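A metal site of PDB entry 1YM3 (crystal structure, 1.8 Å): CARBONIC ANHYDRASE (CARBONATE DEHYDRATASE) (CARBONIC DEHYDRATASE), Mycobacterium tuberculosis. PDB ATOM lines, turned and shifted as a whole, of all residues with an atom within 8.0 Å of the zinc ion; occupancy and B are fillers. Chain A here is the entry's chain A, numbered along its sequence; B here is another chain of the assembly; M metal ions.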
ATOM      1  N   GLY A  58      14.725  18.543  -7.549  1.00  0.00           N
ATOM      2  CA  GLY A  58      14.025  17.575  -8.362  1.00  0.00           C
ATOM      3  C   GLY A  58      14.661  16.224  -8.565  1.00  0.00           C
ATOM      4  O   GLY A  58      15.728  15.928  -8.058  1.00  0.00           O
ATOM      5  N   CYS A  59      13.957  15.382  -9.314  1.00  0.00           N
ATOM      6  CA  CYS A  59      14.403  14.008  -9.584  1.00  0.00           C
ATOM      7  C   CYS A  59      15.140  13.936 -10.925  1.00  0.00           C
ATOM      8  O   CYS A  59      14.685  14.500 -11.952  1.00  0.00           O
ATOM      9  CB  CYS A  59      13.221  12.992  -9.558  1.00  0.00           C
ATOM     10  SG  CYS A  59      13.806  11.291  -9.814  1.00  0.00           S
ATOM     11  N   ALA A  60      16.217  13.163 -10.955  1.00  0.00           N
ATOM     12  CA  ALA A  60      17.042  13.042 -12.147  1.00  0.00           C
ATOM     13  C   ALA A  60      16.319  12.383 -13.282  1.00  0.00           C
ATOM     14  O   ALA A  60      16.664  12.625 -14.464  1.00  0.00           O
ATOM     15  CB  ALA A  60      18.364  12.293 -11.845  1.00  0.00           C
ATOM     16  N   ASP A  61      15.300  11.548 -12.979  1.00  0.00           N
ATOM     17  CA  ASP A  61      14.520  10.895 -14.066  1.00  0.00           C
ATOM     18  C   ASP A  61      13.247  11.604 -14.496  1.00  0.00           C
ATOM     19  O   ASP A  61      12.467  11.063 -15.296  1.00  0.00           O
ATOM     20  CB  ASP A  61      14.349   9.376 -13.818  1.00  0.00           C
ATOM     21  CG  ASP A  61      13.463   9.045 -12.693  1.00  0.00           C
ATOM     22  OD1 ASP A  61      12.449   9.737 -12.508  1.00  0.00           O
ATOM     23  OD2 ASP A  61      13.712   8.059 -11.940  1.00  0.00           O
ATOM     24  N   SER A  62      13.055  12.830 -14.015  1.00  0.00           N
ATOM     25  CA  SER A  62      12.012  13.714 -14.522  1.00  0.00           C
ATOM     26  C   SER A  62      12.211  13.866 -16.023  1.00  0.00           C
ATOM     27  O   SER A  62      13.348  13.795 -16.523  1.00  0.00           O
ATOM     28  CB  SER A  62      12.043  15.058 -13.765  1.00  0.00           C
ATOM     29  OG  SER A  62      11.446  16.087 -14.540  1.00  0.00           O
ATOM     30  N   ARG A  63      11.110  14.030 -16.740  1.00  0.00           N
ATOM     31  CA  ARG A  63      11.130  14.079 -18.186  1.00  0.00           C
ATOM     32  C   ARG A  63      11.123  15.491 -18.752  1.00  0.00           C
ATOM     33  O   ARG A  63      11.296  15.665 -19.964  1.00  0.00           O
ATOM     34  CB  ARG A  63       9.936  13.287 -18.732  1.00  0.00           C
ATOM     35  CG  ARG A  63      10.115  11.820 -18.494  1.00  0.00           C
ATOM     36  CD  ARG A  63       8.919  10.934 -18.775  1.00  0.00           C
ATOM     37  NE  ARG A  63       8.185  10.654 -17.561  1.00  0.00           N
ATOM     38  CZ  ARG A  63       8.638   9.978 -16.476  1.00  0.00           C
ATOM     39  NH1 ARG A  63       9.880   9.424 -16.431  1.00  0.00           N
ATOM     40  NH2 ARG A  63       7.847   9.848 -15.428  1.00  0.00           N
ATOM     41  N   ARG A  81      19.385  18.204  -8.533  1.00  0.00           N
ATOM     42  CA  ARG A  81      18.666  17.019  -9.010  1.00  0.00           C
ATOM     43  C   ARG A  81      19.455  15.762  -8.681  1.00  0.00           C
ATOM     44  O   ARG A  81      20.647  15.668  -9.024  1.00  0.00           O
ATOM     45  CB  ARG A  81      18.464  17.071 -10.516  1.00  0.00           C
ATOM     46  CG  ARG A  81      17.233  17.740 -10.948  1.00  0.00           C
ATOM     47  CD  ARG A  81      16.931  17.633 -12.423  1.00  0.00           C
ATOM     48  NE  ARG A  81      15.945  18.645 -12.690  1.00  0.00           N
ATOM     49  CZ  ARG A  81      14.662  18.529 -12.454  1.00  0.00           C
ATOM     50  NH1 ARG A  81      14.140  17.376 -12.007  1.00  0.00           N
ATOM     51  NH2 ARG A  81      13.859  19.582 -12.628  1.00  0.00           N
ATOM     52  N   THR A  82      18.796  14.771  -8.074  1.00  0.00           N
ATOM     53  CA  THR A  82      19.381  13.434  -7.874  1.00  0.00           C
ATOM     54  C   THR A  82      18.311  12.380  -8.145  1.00  0.00           C
ATOM     55  O   THR A  82      17.118  12.691  -8.144  1.00  0.00           O
ATOM     56  CB  THR A  82      19.945  13.226  -6.409  1.00  0.00           C
ATOM     57  OG1 THR A  82      18.867  13.361  -5.447  1.00  0.00           O
ATOM     58  CG2 THR A  82      21.029  14.169  -6.061  1.00  0.00           C
ATOM     59  N   ALA A  83      18.733  11.124  -8.325  1.00  0.00           N
ATOM     60  CA  ALA A  83      17.782  10.032  -8.545  1.00  0.00           C
ATOM     61  C   ALA A  83      16.927   9.811  -7.303  1.00  0.00           C
ATOM     62  O   ALA A  83      17.453   9.609  -6.220  1.00  0.00           O
ATOM     63  CB  ALA A  83      18.501   8.741  -8.944  1.00  0.00           C
ATOM     64  N   GLY A  84      15.612   9.938  -7.439  1.00  0.00           N
ATOM     65  CA  GLY A  84      14.734   9.748  -6.286  1.00  0.00           C
ATOM     66  C   GLY A  84      14.832  10.784  -5.179  1.00  0.00           C
ATOM     67  O   GLY A  84      14.516  10.462  -4.033  1.00  0.00           O
ATOM     68  N   HIS A  85      15.309  11.987  -5.476  1.00  0.00           N
ATOM     69  CA  HIS A  85      15.514  13.007  -4.446  1.00  0.00           C
ATOM     70  C   HIS A  85      16.410  12.550  -3.307  1.00  0.00           C
ATOM     71  O   HIS A  85      16.266  13.070  -2.196  1.00  0.00           O
ATOM     72  CB  HIS A  85      14.173  13.451  -3.809  1.00  0.00           C
ATOM     73  CG  HIS A  85      13.256  14.102  -4.789  1.00  0.00           C
ATOM     74  ND1 HIS A  85      12.396  13.402  -5.590  1.00  0.00           N
ATOM     75  CD2 HIS A  85      13.073  15.404  -5.072  1.00  0.00           C
ATOM     76  CE1 HIS A  85      11.723  14.247  -6.346  1.00  0.00           C
ATOM     77  NE2 HIS A  85      12.151  15.475  -6.077  1.00  0.00           N
ATOM     78  N   LEU A 110      10.327  19.006  -5.668  1.00  0.00           N
ATOM     79  CA  LEU A 110       9.418  18.835  -6.781  1.00  0.00           C
ATOM     80  C   LEU A 110       9.353  17.374  -7.173  1.00  0.00           C
ATOM     81  O   LEU A 110      10.338  16.834  -7.719  1.00  0.00           O
ATOM     82  CB  LEU A 110       9.881  19.678  -7.959  1.00  0.00           C
ATOM     83  CG  LEU A 110       9.057  19.684  -9.223  1.00  0.00           C
ATOM     84  CD1 LEU A 110       7.626  20.206  -8.997  1.00  0.00           C
ATOM     85  CD2 LEU A 110       9.806  20.483 -10.247  1.00  0.00           C
ATOM     86  N   GLY A 111       8.201  16.754  -6.952  1.00  0.00           N
ATOM     87  CA  GLY A 111       7.980  15.359  -7.374  1.00  0.00           C
ATOM     88  C   GLY A 111       7.183  15.256  -8.669  1.00  0.00           C
ATOM     89  O   GLY A 111       6.652  16.249  -9.192  1.00  0.00           O
ATOM     90  N   HIS A 112       7.093  14.043  -9.184  1.00  0.00           N
ATOM     91  CA  HIS A 112       6.556  13.786 -10.528  1.00  0.00           C
ATOM     92  C   HIS A 112       5.949  12.396 -10.617  1.00  0.00           C
ATOM     93  O   HIS A 112       6.274  11.503  -9.822  1.00  0.00           O
ATOM     94  CB  HIS A 112       7.618  13.997 -11.630  1.00  0.00           C
ATOM     95  CG  HIS A 112       8.696  12.936 -11.701  1.00  0.00           C
ATOM     96  ND1 HIS A 112       8.975  12.252 -12.861  1.00  0.00           N
ATOM     97  CD2 HIS A 112       9.595  12.465 -10.777  1.00  0.00           C
ATOM     98  CE1 HIS A 112       9.961  11.383 -12.644  1.00  0.00           C
ATOM     99  NE2 HIS A 112      10.338  11.462 -11.381  1.00  0.00           N
ATOM    100  N   ASP A 113       5.083  12.238 -11.629  1.00  0.00           N
ATOM    101  CA  ASP A 113       4.488  10.953 -11.945  1.00  0.00           C
ATOM    102  C   ASP A 113       5.440   9.902 -12.553  1.00  0.00           C
ATOM    103  O   ASP A 113       6.444  10.233 -13.214  1.00  0.00           O
ATOM    104  CB  ASP A 113       3.227  11.134 -12.819  1.00  0.00           C
ATOM    105  CG  ASP A 113       3.554  11.594 -14.220  1.00  0.00           C
ATOM    106  OD1 ASP A 113       4.265  12.624 -14.383  1.00  0.00           O
ATOM    107  OD2 ASP A 113       3.144  10.974 -15.246  1.00  0.00           O
ATOM    108  N   SER A 114       5.099   8.639 -12.331  1.00  0.00           N
ATOM    109  CA  SER A 114       5.817   7.505 -12.873  1.00  0.00           C
ATOM    110  C   SER A 114       7.327   7.593 -12.629  1.00  0.00           C
ATOM    111  O   SER A 114       8.148   7.453 -13.541  1.00  0.00           O
ATOM    112  CB  SER A 114       5.508   7.383 -14.362  1.00  0.00           C
ATOM    113  OG  SER A 114       4.179   6.922 -14.494  1.00  0.00           O
ATOM    114  N   CYS A 115       7.676   7.873 -11.383  1.00  0.00           N
ATOM    115  CA  CYS A 115       9.072   7.985 -11.006  1.00  0.00           C
ATOM    116  C   CYS A 115       9.740   6.606 -11.013  1.00  0.00           C
ATOM    117  O   CYS A 115       9.359   5.710 -10.242  1.00  0.00           O
ATOM    118  CB  CYS A 115       9.205   8.593  -9.596  1.00  0.00           C
ATOM    119  SG  CYS A 115      10.946   8.785  -9.069  1.00  0.00           S
ATOM    120  N   GLY A 116      10.737   6.435 -11.888  1.00  0.00           N
ATOM    121  CA  GLY A 116      11.426   5.167 -11.948  1.00  0.00           C
ATOM    122  C   GLY A 116      12.261   4.830 -10.730  1.00  0.00           C
ATOM    123  O   GLY A 116      12.343   3.679 -10.372  1.00  0.00           O
ATOM    124  N   ALA A 117      12.887   5.835 -10.080  1.00  0.00           N
ATOM    125  CA  ALA A 117      13.660   5.556  -8.892  1.00  0.00           C
ATOM    126  C   ALA A 117      12.786   4.986  -7.770  1.00  0.00           C
ATOM    127  O   ALA A 117      13.176   4.074  -7.057  1.00  0.00           O
ATOM    128  CB  ALA A 117      14.356   6.824  -8.400  1.00  0.00           C
ATOM    129  N   VAL A 118      11.597   5.546  -7.613  1.00  0.00           N
ATOM    130  CA  VAL A 118      10.677   5.011  -6.609  1.00  0.00           C
ATOM    131  C   VAL A 118      10.280   3.563  -6.977  1.00  0.00           C
ATOM    132  O   VAL A 118      10.257   2.672  -6.107  1.00  0.00           O
ATOM    133  CB  VAL A 118       9.478   5.970  -6.397  1.00  0.00           C
ATOM    134  CG1 VAL A 118       8.410   5.326  -5.574  1.00  0.00           C
ATOM    135  CG2 VAL A 118       9.976   7.263  -5.736  1.00  0.00           C
ATOM    136  N   ASN A 119      10.036   3.297  -8.253  1.00  0.00           N
ATOM    137  CA  ASN A 119       9.708   1.946  -8.694  1.00  0.00           C
ATOM    138  C   ASN A 119      10.859   0.951  -8.449  1.00  0.00           C
ATOM    139  O   ASN A 119      10.618  -0.199  -8.098  1.00  0.00           O
ATOM    140  CB  ASN A 119       9.267   1.944 -10.178  1.00  0.00           C
ATOM    141  CG  ASN A 119       8.473   0.726 -10.552  1.00  0.00           C
ATOM    142  OD1 ASN A 119       8.853  -0.016 -11.437  1.00  0.00           O
ATOM    143  ND2 ASN A 119       7.381   0.476  -9.835  1.00  0.00           N
ATOM    144  N   VAL A 157       2.941   3.669  -7.215  1.00  0.00           N
ATOM    145  CA  VAL A 157       4.174   4.442  -7.336  1.00  0.00           C
ATOM    146  C   VAL A 157       3.923   5.916  -7.041  1.00  0.00           C
ATOM    147  O   VAL A 157       4.707   6.540  -6.309  1.00  0.00           O
ATOM    148  CB  VAL A 157       4.847   4.245  -8.725  1.00  0.00           C
ATOM    149  CG1 VAL A 157       5.932   5.317  -9.039  1.00  0.00           C
ATOM    150  CG2 VAL A 157       5.449   2.857  -8.825  1.00  0.00           C
ATOM    151  N   GLU A 161       5.551   8.326  -4.159  1.00  0.00           N
ATOM    152  CA  GLU A 161       6.368   9.497  -4.543  1.00  0.00           C
ATOM    153  C   GLU A 161       5.899  10.730  -3.779  1.00  0.00           C
ATOM    154  O   GLU A 161       6.718  11.491  -3.242  1.00  0.00           O
ATOM    155  CB  GLU A 161       6.340   9.722  -6.081  1.00  0.00           C
ATOM    156  CG  GLU A 161       6.745  11.117  -6.557  1.00  0.00           C
ATOM    157  CD  GLU A 161       8.232  11.319  -6.597  1.00  0.00           C
ATOM    158  OE1 GLU A 161       8.946  10.519  -5.898  1.00  0.00           O
ATOM    159  OE2 GLU A 161       8.671  12.227  -7.353  1.00  0.00           O
ATOM    160  N   TYR A 195       3.671  17.162  -9.861  1.00  0.00           N
ATOM    161  CA  TYR A 195       2.862  17.302 -11.086  1.00  0.00           C
ATOM    162  C   TYR A 195       2.725  15.974 -11.804  1.00  0.00           C
ATOM    163  O   TYR A 195       3.455  15.048 -11.511  1.00  0.00           O
ATOM    164  CB  TYR A 195       3.491  18.346 -11.998  1.00  0.00           C
ATOM    165  CG  TYR A 195       4.843  17.932 -12.494  1.00  0.00           C
ATOM    166  CD1 TYR A 195       4.987  17.414 -13.771  1.00  0.00           C
ATOM    167  CD2 TYR A 195       5.964  18.037 -11.703  1.00  0.00           C
ATOM    168  CE1 TYR A 195       6.231  16.989 -14.260  1.00  0.00           C
ATOM    169  CE2 TYR A 195       7.250  17.638 -12.184  1.00  0.00           C
ATOM    170  CZ  TYR A 195       7.356  17.092 -13.482  1.00  0.00           C
ATOM    171  OH  TYR A 195       8.580  16.662 -14.006  1.00  0.00           O
ATOM    172  N   PHE B  78      18.702  12.278 -18.588  1.00  0.00           N
ATOM    173  CA  PHE B  78      18.689  11.988 -17.163  1.00  0.00           C
ATOM    174  C   PHE B  78      19.664  12.984 -16.594  1.00  0.00           C
ATOM    175  O   PHE B  78      20.842  12.991 -16.945  1.00  0.00           O
ATOM    176  CB  PHE B  78      19.109  10.522 -16.957  1.00  0.00           C
ATOM    177  CG  PHE B  78      19.190  10.037 -15.525  1.00  0.00           C
ATOM    178  CD1 PHE B  78      18.148   9.261 -14.970  1.00  0.00           C
ATOM    179  CD2 PHE B  78      20.328  10.292 -14.735  1.00  0.00           C
ATOM    180  CE1 PHE B  78      18.228   8.777 -13.704  1.00  0.00           C
ATOM    181  CE2 PHE B  78      20.434   9.779 -13.418  1.00  0.00           C
ATOM    182  CZ  PHE B  78      19.353   9.013 -12.907  1.00  0.00           C
ATOM    183  N   TYR B  97      23.238   4.478 -11.344  1.00  0.00           N
ATOM    184  CA  TYR B  97      21.901   3.972 -11.628  1.00  0.00           C
ATOM    185  C   TYR B  97      21.495   4.150 -13.099  1.00  0.00           C
ATOM    186  O   TYR B  97      20.977   3.204 -13.720  1.00  0.00           O
ATOM    187  CB  TYR B  97      20.907   4.632 -10.665  1.00  0.00           C
ATOM    188  CG  TYR B  97      19.435   4.416 -11.016  1.00  0.00           C
ATOM    189  CD1 TYR B  97      18.742   3.319 -10.549  1.00  0.00           C
ATOM    190  CD2 TYR B  97      18.771   5.323 -11.826  1.00  0.00           C
ATOM    191  CE1 TYR B  97      17.423   3.127 -10.880  1.00  0.00           C
ATOM    192  CE2 TYR B  97      17.477   5.155 -12.169  1.00  0.00           C
ATOM    193  CZ  TYR B  97      16.781   4.066 -11.660  1.00  0.00           C
ATOM    194  OH  TYR B  97      15.482   3.865 -11.991  1.00  0.00           O
HETATM  195 ZN    ZN M   1      11.803  10.285 -10.586  1.00  0.00          ZN
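Four residues have an atom within 4 Å of the zinc ion: Cys 59, Asp 61, His 112 and Cys 115.
O of Cys 59 is in hydrogen-bond range of NH1 of Arg 81, at 2.9 Å. The side-chain carboxylate (OD2) of Asp 61 sits at hydrogen-bond distance from the backbone NH (N) of Ala 117 (3.0 Å). SG of Cys 59 lies close to N of Gly 84 (3.3 Å). OE2 of Glu 161 is in hydrogen-bond range of N of His 112 (3.0 Å). O of Asp 61 is in hydrogen-bond range of NH1 of Arg 63 (3.3 Å). The backbone NH (N) of Val 118 sits close to the side-chain sulfur (SG) of Cys 115. The side-chain sulfur (SG) of Cys 115 lies close to the backbone NH (N) of Ala 117, 3.7 Å away. OD2 of Asp 61 is in hydrogen-bond range of N of Gly 116 (3.4 Å).
The zinc ion is bound by NE2 of His 112, OD1 of Asp 61, SG of Cys 115 and SG of Cys 59. The zinc ion has four donor atoms within binding distance.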
